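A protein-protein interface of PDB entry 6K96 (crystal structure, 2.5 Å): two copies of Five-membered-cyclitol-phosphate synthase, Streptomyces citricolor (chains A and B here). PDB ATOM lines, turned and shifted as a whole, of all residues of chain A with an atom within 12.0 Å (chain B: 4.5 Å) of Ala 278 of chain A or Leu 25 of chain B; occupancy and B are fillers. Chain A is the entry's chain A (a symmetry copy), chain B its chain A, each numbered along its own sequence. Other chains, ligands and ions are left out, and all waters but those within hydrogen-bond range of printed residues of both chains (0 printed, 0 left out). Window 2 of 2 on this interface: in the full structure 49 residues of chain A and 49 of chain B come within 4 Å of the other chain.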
ATOM      1  N   ARG A 204       8.254  -4.673  39.166  1.00  0.00           N
ATOM      2  CA  ARG A 204       8.196  -3.603  38.121  1.00  0.00           C
ATOM      3  C   ARG A 204       8.607  -4.192  36.773  1.00  0.00           C
ATOM      4  O   ARG A 204       8.468  -3.478  35.758  1.00  0.00           O
ATOM      5  CB  ARG A 204       9.048  -2.357  38.442  1.00  0.00           C
ATOM      6  CG  ARG A 204       9.154  -1.973  39.917  1.00  0.00           C
ATOM      7  CD  ARG A 204       8.425  -0.814  40.545  1.00  0.00           C
ATOM      8  NE  ARG A 204       8.344   0.300  39.614  1.00  0.00           N
ATOM      9  CZ  ARG A 204       7.461   1.317  39.704  1.00  0.00           C
ATOM     10  NH1 ARG A 204       6.648   1.418  40.756  1.00  0.00           N
ATOM     11  NH2 ARG A 204       7.412   2.252  38.754  1.00  0.00           N
ATOM     12  N   GLY A 205       9.064  -5.434  36.720  1.00  0.00           N
ATOM     13  CA  GLY A 205       9.267  -6.064  35.405  1.00  0.00           C
ATOM     14  C   GLY A 205      10.675  -5.870  34.896  1.00  0.00           C
ATOM     15  O   GLY A 205      10.923  -6.197  33.781  1.00  0.00           O
ATOM     16  N   LEU A 206      11.615  -5.536  35.764  1.00  0.00           N
ATOM     17  CA  LEU A 206      13.057  -5.576  35.410  1.00  0.00           C
ATOM     18  C   LEU A 206      13.540  -7.026  35.441  1.00  0.00           C
ATOM     19  O   LEU A 206      12.954  -7.832  36.175  1.00  0.00           O
ATOM     20  CB  LEU A 206      13.850  -4.656  36.346  1.00  0.00           C
ATOM     21  CG  LEU A 206      13.548  -3.183  36.100  1.00  0.00           C
ATOM     22  CD1 LEU A 206      12.400  -2.725  36.957  1.00  0.00           C
ATOM     23  CD2 LEU A 206      14.735  -2.294  36.310  1.00  0.00           C
ATOM     24  N   SER A 207      14.494  -7.361  34.573  1.00  0.00           N
ATOM     25  CA  SER A 207      15.152  -8.703  34.577  1.00  0.00           C
ATOM     26  C   SER A 207      16.368  -8.701  35.510  1.00  0.00           C
ATOM     27  O   SER A 207      17.097  -7.674  35.523  1.00  0.00           O
ATOM     28  CB  SER A 207      15.512  -9.092  33.174  1.00  0.00           C
ATOM     29  OG  SER A 207      14.327  -9.219  32.414  1.00  0.00           O
ATOM     30  N   ALA A 209      20.039  -9.946  36.112  1.00  0.00           N
ATOM     31  CA  ALA A 209      21.232 -10.519  35.449  1.00  0.00           C
ATOM     32  C   ALA A 209      22.030 -11.322  36.487  1.00  0.00           C
ATOM     33  O   ALA A 209      22.503 -12.447  36.175  1.00  0.00           O
ATOM     34  CB  ALA A 209      22.102  -9.431  34.858  1.00  0.00           C
ATOM     35  N   GLY A 274      20.336  -5.489  37.449  1.00  0.00           N
ATOM     36  CA  GLY A 274      19.094  -5.708  36.690  1.00  0.00           C
ATOM     37  C   GLY A 274      19.234  -5.304  35.236  1.00  0.00           C
ATOM     38  O   GLY A 274      20.270  -4.702  34.841  1.00  0.00           O
ATOM     39  N   LEU A 275      18.227  -5.629  34.438  1.00  0.00           N
ATOM     40  CA  LEU A 275      18.184  -5.148  33.051  1.00  0.00           C
ATOM     41  C   LEU A 275      16.821  -4.549  32.837  1.00  0.00           C
ATOM     42  O   LEU A 275      15.841  -5.184  33.245  1.00  0.00           O
ATOM     43  CB  LEU A 275      18.446  -6.293  32.067  1.00  0.00           C
ATOM     44  CG  LEU A 275      19.768  -7.040  32.232  1.00  0.00           C
ATOM     45  CD1 LEU A 275      19.670  -8.340  31.481  1.00  0.00           C
ATOM     46  CD2 LEU A 275      20.933  -6.209  31.730  1.00  0.00           C
ATOM     47  N   GLY A 276      16.842  -3.357  32.240  1.00  0.00           N
ATOM     48  CA  GLY A 276      15.704  -2.435  32.061  1.00  0.00           C
ATOM     49  C   GLY A 276      15.256  -2.469  30.630  1.00  0.00           C
ATOM     50  O   GLY A 276      15.727  -3.342  29.882  1.00  0.00           O
ATOM     51  N   TRP A 277      14.371  -1.557  30.254  1.00  0.00           N
ATOM     52  CA  TRP A 277      13.965  -1.380  28.847  1.00  0.00           C
ATOM     53  C   TRP A 277      15.183  -1.489  27.931  1.00  0.00           C
ATOM     54  O   TRP A 277      16.191  -0.870  28.203  1.00  0.00           O
ATOM     55  CB  TRP A 277      13.252  -0.028  28.707  1.00  0.00           C
ATOM     56  CG  TRP A 277      12.935   0.368  27.297  1.00  0.00           C
ATOM     57  CD1 TRP A 277      13.670   1.182  26.509  1.00  0.00           C
ATOM     58  CD2 TRP A 277      11.901  -0.180  26.484  1.00  0.00           C
ATOM     59  NE1 TRP A 277      13.124   1.222  25.277  1.00  0.00           N
ATOM     60  CE2 TRP A 277      12.029   0.418  25.232  1.00  0.00           C
ATOM     61  CE3 TRP A 277      10.890  -1.119  26.700  1.00  0.00           C
ATOM     62  CZ2 TRP A 277      11.142   0.166  24.196  1.00  0.00           C
ATOM     63  CZ3 TRP A 277      10.001  -1.368  25.685  1.00  0.00           C
ATOM     64  CH2 TRP A 277      10.145  -0.744  24.444  1.00  0.00           C
ATOM     65  N   ALA A 278      15.095  -2.295  26.885  1.00  0.00           N
ATOM     66  CA  ALA A 278      16.128  -2.371  25.833  1.00  0.00           C
ATOM     67  C   ALA A 278      17.387  -3.087  26.308  1.00  0.00           C
ATOM     68  O   ALA A 278      18.425  -2.952  25.606  1.00  0.00           O
ATOM     69  CB  ALA A 278      16.496  -0.965  25.423  1.00  0.00           C
ATOM     70  N   GLY A 279      17.324  -3.784  27.450  1.00  0.00           N
ATOM     71  CA  GLY A 279      18.480  -4.409  28.082  1.00  0.00           C
ATOM     72  C   GLY A 279      19.464  -3.405  28.654  1.00  0.00           C
ATOM     73  O   GLY A 279      20.621  -3.824  28.887  1.00  0.00           O
ATOM     74  N   THR A 280      19.078  -2.172  28.992  1.00  0.00           N
ATOM     75  CA  THR A 280      20.024  -1.243  29.671  1.00  0.00           C
ATOM     76  C   THR A 280      20.209  -1.663  31.127  1.00  0.00           C
ATOM     77  O   THR A 280      19.282  -2.167  31.758  1.00  0.00           O
ATOM     78  CB  THR A 280      19.611   0.220  29.556  1.00  0.00           C
ATOM     79  OG1 THR A 280      18.552   0.452  30.487  1.00  0.00           O
ATOM     80  CG2 THR A 280      19.278   0.591  28.128  1.00  0.00           C
ATOM     81  N   PRO A 281      21.431  -1.555  31.690  1.00  0.00           N
ATOM     82  CA  PRO A 281      21.678  -2.020  33.055  1.00  0.00           C
ATOM     83  C   PRO A 281      21.067  -1.110  34.132  1.00  0.00           C
ATOM     84  O   PRO A 281      21.120   0.105  34.045  1.00  0.00           O
ATOM     85  CB  PRO A 281      23.187  -1.990  33.219  1.00  0.00           C
ATOM     86  CG  PRO A 281      23.710  -1.912  31.776  1.00  0.00           C
ATOM     87  CD  PRO A 281      22.666  -1.114  31.016  1.00  0.00           C
ATOM     88  N   VAL A 282      20.545  -1.767  35.154  1.00  0.00           N
ATOM     89  CA  VAL A 282      20.148  -1.155  36.439  1.00  0.00           C
ATOM     90  C   VAL A 282      21.117  -1.749  37.434  1.00  0.00           C
ATOM     91  O   VAL A 282      21.119  -2.942  37.502  1.00  0.00           O
ATOM     92  CB  VAL A 282      18.670  -1.495  36.706  1.00  0.00           C
ATOM     93  CG1 VAL A 282      18.236  -1.361  38.151  1.00  0.00           C
ATOM     94  CG2 VAL A 282      17.806  -0.642  35.785  1.00  0.00           C
ATOM     95  N   GLN B  21      14.701   3.168  19.237  1.00  0.00           N
ATOM     96  CA  GLN B  21      15.795   2.145  19.264  1.00  0.00           C
ATOM     97  C   GLN B  21      15.332   0.911  20.039  1.00  0.00           C
ATOM     98  O   GLN B  21      15.620  -0.208  19.607  1.00  0.00           O
ATOM     99  CB  GLN B  21      17.053   2.671  19.948  1.00  0.00           C
ATOM    100  CG  GLN B  21      17.700   3.813  19.218  1.00  0.00           C
ATOM    101  CD  GLN B  21      19.139   4.011  19.621  1.00  0.00           C
ATOM    102  OE1 GLN B  21      20.017   3.270  19.168  1.00  0.00           O
ATOM    103  NE2 GLN B  21      19.395   5.031  20.433  1.00  0.00           N
ATOM    104  N   GLY B  22      14.681   1.097  21.180  1.00  0.00           N
ATOM    105  CA  GLY B  22      14.263  -0.041  22.022  1.00  0.00           C
ATOM    106  C   GLY B  22      13.408  -0.980  21.208  1.00  0.00           C
ATOM    107  O   GLY B  22      13.801  -2.120  21.059  1.00  0.00           O
ATOM    108  N   ALA B  23      12.333  -0.458  20.603  1.00  0.00           N
ATOM    109  CA  ALA B  23      11.353  -1.234  19.809  1.00  0.00           C
ATOM    110  C   ALA B  23      12.072  -2.083  18.758  1.00  0.00           C
ATOM    111  O   ALA B  23      11.616  -3.212  18.566  1.00  0.00           O
ATOM    112  CB  ALA B  23      10.322  -0.326  19.157  1.00  0.00           C
ATOM    113  N   GLU B  24      13.107  -1.560  18.078  1.00  0.00           N
ATOM    114  CA  GLU B  24      13.831  -2.331  17.022  1.00  0.00           C
ATOM    115  C   GLU B  24      14.840  -3.296  17.620  1.00  0.00           C
ATOM    116  O   GLU B  24      15.212  -4.231  16.901  1.00  0.00           O
ATOM    117  CB  GLU B  24      14.644  -1.488  16.050  1.00  0.00           C
ATOM    118  CG  GLU B  24      13.813  -0.527  15.226  1.00  0.00           C
ATOM    119  CD  GLU B  24      12.393  -0.909  14.835  1.00  0.00           C
ATOM    120  OE1 GLU B  24      12.215  -2.064  14.330  1.00  0.00           O
ATOM    121  OE2 GLU B  24      11.466  -0.019  15.013  1.00  0.00           O
ATOM    122  N   LEU B  25      15.304  -3.068  18.850  1.00  0.00           N
ATOM    123  CA  LEU B  25      16.144  -4.072  19.539  1.00  0.00           C
ATOM    124  C   LEU B  25      15.266  -5.300  19.818  1.00  0.00           C
ATOM    125  O   LEU B  25      15.692  -6.375  19.457  1.00  0.00           O
ATOM    126  CB  LEU B  25      16.785  -3.493  20.804  1.00  0.00           C
ATOM    127  CG  LEU B  25      17.746  -4.438  21.527  1.00  0.00           C
ATOM    128  CD1 LEU B  25      18.871  -4.903  20.617  1.00  0.00           C
ATOM    129  CD2 LEU B  25      18.324  -3.792  22.769  1.00  0.00           C
ATOM    130  N   TYR B  26      14.077  -5.152  20.395  1.00  0.00           N
ATOM    131  CA  TYR B  26      13.155  -6.288  20.639  1.00  0.00           C
ATOM    132  C   TYR B  26      12.743  -6.936  19.318  1.00  0.00           C
ATOM    133  O   TYR B  26      12.537  -8.120  19.322  1.00  0.00           O
ATOM    134  CB  TYR B  26      11.929  -5.883  21.447  1.00  0.00           C
ATOM    135  CG  TYR B  26      12.292  -5.486  22.845  1.00  0.00           C
ATOM    136  CD1 TYR B  26      12.777  -6.431  23.730  1.00  0.00           C
ATOM    137  CD2 TYR B  26      12.160  -4.185  23.283  1.00  0.00           C
ATOM    138  CE1 TYR B  26      13.146  -6.093  25.018  1.00  0.00           C
ATOM    139  CE2 TYR B  26      12.485  -3.830  24.579  1.00  0.00           C
ATOM    140  CZ  TYR B  26      13.019  -4.789  25.446  1.00  0.00           C
ATOM    141  OH  TYR B  26      13.353  -4.524  26.748  1.00  0.00           O
ATOM    142  N   ARG B  27      12.605  -6.190  18.226  1.00  0.00           N
ATOM    143  CA  ARG B  27      12.233  -6.790  16.916  1.00  0.00           C
ATOM    144  C   ARG B  27      13.356  -7.744  16.510  1.00  0.00           C
ATOM    145  O   ARG B  27      13.041  -8.813  15.997  1.00  0.00           O
ATOM    146  CB  ARG B  27      12.016  -5.726  15.829  1.00  0.00           C
ATOM    147  CG  ARG B  27      10.717  -5.921  15.059  1.00  0.00           C
ATOM    148  CD  ARG B  27      10.564  -5.062  13.830  1.00  0.00           C
ATOM    149  NE  ARG B  27      10.488  -3.665  14.235  1.00  0.00           N
ATOM    150  CZ  ARG B  27       9.402  -3.061  14.725  1.00  0.00           C
ATOM    151  NH1 ARG B  27       8.277  -3.737  14.882  1.00  0.00           N
ATOM    152  NH2 ARG B  27       9.460  -1.796  15.102  1.00  0.00           N
ATOM    153  N   LYS B  28      14.608  -7.333  16.723  1.00  0.00           N
ATOM    154  CA  LYS B  28      15.847  -8.063  16.339  1.00  0.00           C
ATOM    155  C   LYS B  28      15.942  -9.332  17.185  1.00  0.00           C
ATOM    156  O   LYS B  28      16.266 -10.359  16.630  1.00  0.00           O
ATOM    157  CB  LYS B  28      17.079  -7.157  16.490  1.00  0.00           C
ATOM    158  CG  LYS B  28      18.421  -7.883  16.611  1.00  0.00           C
ATOM    159  CD  LYS B  28      19.581  -6.974  16.949  1.00  0.00           C
ATOM    160  CE  LYS B  28      20.774  -7.726  17.504  1.00  0.00           C
ATOM    161  NZ  LYS B  28      21.653  -8.232  16.419  1.00  0.00           N
ATOM    162  N   MET B  29      15.665  -9.247  18.483  1.00  0.00           N
ATOM    163  CA  MET B  29      15.668 -10.410  19.417  1.00  0.00           C
ATOM    164  C   MET B  29      14.625 -11.448  18.967  1.00  0.00           C
ATOM    165  O   MET B  29      14.886 -12.663  19.150  1.00  0.00           O
ATOM    166  CB  MET B  29      15.376  -9.991  20.867  1.00  0.00           C
ATOM    167  CG  MET B  29      16.509  -9.251  21.556  1.00  0.00           C
ATOM    168  SD  MET B  29      16.012  -9.005  23.250  1.00  0.00           S
ATOM    169  CE  MET B  29      17.523  -8.501  24.079  1.00  0.00           C
ATOM    170  N   PRO B  40      14.109  -8.703  28.250  1.00  0.00           N
ATOM    171  CA  PRO B  40      14.577  -7.949  29.406  1.00  0.00           C
ATOM    172  C   PRO B  40      13.811  -6.636  29.601  1.00  0.00           C
ATOM    173  O   PRO B  40      13.695  -5.860  28.666  1.00  0.00           O
ATOM    174  CB  PRO B  40      16.038  -7.646  29.056  1.00  0.00           C
ATOM    175  CG  PRO B  40      16.043  -7.590  27.547  1.00  0.00           C
ATOM    176  CD  PRO B  40      15.085  -8.692  27.153  1.00  0.00           C
ATOM    177  N   TYR B  83      21.068   9.603  24.755  1.00  0.00           N
ATOM    178  CA  TYR B  83      20.746   8.171  24.906  1.00  0.00           C
ATOM    179  C   TYR B  83      21.716   7.422  24.011  1.00  0.00           C
ATOM    180  O   TYR B  83      22.058   7.920  22.949  1.00  0.00           O
ATOM    181  CB  TYR B  83      19.318   7.793  24.512  1.00  0.00           C
ATOM    182  CG  TYR B  83      18.883   6.420  24.990  1.00  0.00           C
ATOM    183  CD1 TYR B  83      18.551   6.176  26.312  1.00  0.00           C
ATOM    184  CD2 TYR B  83      18.767   5.367  24.107  1.00  0.00           C
ATOM    185  CE1 TYR B  83      18.099   4.940  26.743  1.00  0.00           C
ATOM    186  CE2 TYR B  83      18.331   4.124  24.520  1.00  0.00           C
ATOM    187  CZ  TYR B  83      18.003   3.902  25.844  1.00  0.00           C
ATOM    188  OH  TYR B  83      17.556   2.674  26.243  1.00  0.00           O
ATOM    189  N   LEU B  86      22.207   1.980  20.580  1.00  0.00           N
ATOM    190  CA  LEU B  86      22.016   0.603  21.065  1.00  0.00           C
ATOM    191  C   LEU B  86      22.524  -0.383  20.014  1.00  0.00           C
ATOM    192  O   LEU B  86      22.553  -1.583  20.342  1.00  0.00           O
ATOM    193  CB  LEU B  86      20.542   0.374  21.392  1.00  0.00           C
ATOM    194  CG  LEU B  86      20.072   0.970  22.723  1.00  0.00           C
ATOM    195  CD1 LEU B  86      18.586   0.723  22.910  1.00  0.00           C
ATOM    196  CD2 LEU B  86      20.858   0.397  23.898  1.00  0.00           C
ATOM    197  N   VAL B  88      21.794  -1.334  16.554  1.00  0.00           N
ATOM    198  CA  VAL B  88      20.673  -2.030  15.870  1.00  0.00           C
ATOM    199  C   VAL B  88      20.358  -1.140  14.672  1.00  0.00           C
ATOM    200  O   VAL B  88      20.181   0.092  14.884  1.00  0.00           O
ATOM    201  CB  VAL B  88      19.443  -2.194  16.787  1.00  0.00           C
ATOM    202  CG1 VAL B  88      18.140  -2.271  16.015  1.00  0.00           C
ATOM    203  CG2 VAL B  88      19.568  -3.392  17.710  1.00  0.00           C
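Ser 207 of chain A touches Pro 40 of chain B. CA of Gly 22 of chain B touches NE1 of Trp 277 of chain A (3.7 Å). CZ2 of Trp 277 of chain A touches N of Ala 23 of chain B, at 3.8 Å. CZ3 of Trp 277 of chain A touches CE2 of Tyr 26 of chain B (3.7 Å). Ala 278 of chain A touches Leu 25 of chain B. Tyr 83 of chain B touches Ala 278 of chain A. Ala 278 of chain A touches Leu 86 of chain B (CB to CD1, 3.7 Å). CG2 of Thr 280 of chain A touches OH of Tyr 83 of chain B, at 3.3 Å.
OE1 of Gln 21 of chain B lies within hydrogen-bond range of N of Leu 86 of chain B (2.9 Å). The backbone carbonyl oxygen (O) of Ser 207 of chain A is in hydrogen-bond range of the backbone NH (N) of Leu 275 of chain A.
The side-chain hydroxyl of Tyr 26 of chain B lies within hydrogen-bond range of the backbone NH of Ala 278 of chain A (2.8 Å). The backbone carbonyl oxygen (O) of Pro 40 of chain B sits close to the backbone carbonyl oxygen (O) of Gly 276 of chain A (3.5 Å).
No position is printed for both chains. Of the 10 pairs that touch across the chains among the printed residues, none has its exchanged pair printed and touching as well.
Of the printed residues of chain B, Ser 207 of chain A touches Pro 40 (3.3 Å). Ala 209 of chain A touches none of the printed residues of chain B. Of the printed residues of chain B, Gly 276 of chain A touches Pro 40 (3.5 Å). Of the printed residues of chain B, Trp 277 of chain A touches Gly 22, Ala 23 and Tyr 26. Of chain B, only Leu 25, Tyr 26, Tyr 83 and Leu 86 come within 4 Å of Ala 278 of chain A. Printed residues of chain B within 4 Å of Thr 280 of chain A: Tyr 83 (3.3 Å). Of chain A, only Trp 277 comes within 4 Å of Gly 22 of chain B. Ala 23 of chain B touches one residue of chain A. No residue of chain A comes within 4 Å of Glu 24 of chain B. Leu 25 of chain B touches just one residue of chain A: Ala 278. Of the printed residues of chain A, Tyr 26 of chain B touches Trp 277 and Ala 278. Lys 28 of chain B touches none of the printed residues of chain A. No residue of chain A comes within 4 Å of Met 29 of chain B. Printed residues of chain A within 4 Å of Tyr 83 of chain B: Ala 278 (3.9 Å) and Thr 280 (3.3 Å). The nearest residue of chain B that does not touch Ala 278 of chain A is Gly 22 of chain B (4.2 Å).
Of the 14 printed residues of chain A, 5 touch a printed residue of chain B. Hydrophobic or aromatic side chains of chain A that line the printed part of chain B: Trp 277 and Ala 278. Printed residues of chain B that touch a printed residue of chain A: Gly 22, Ala 23, Leu 25, Tyr 26, Pro 40, Tyr 83 and Leu 86. Among the printed residues, no Asp or Glu carboxylate lies within 4 Å of a Lys or Arg side-chain nitrogen of the other chain.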
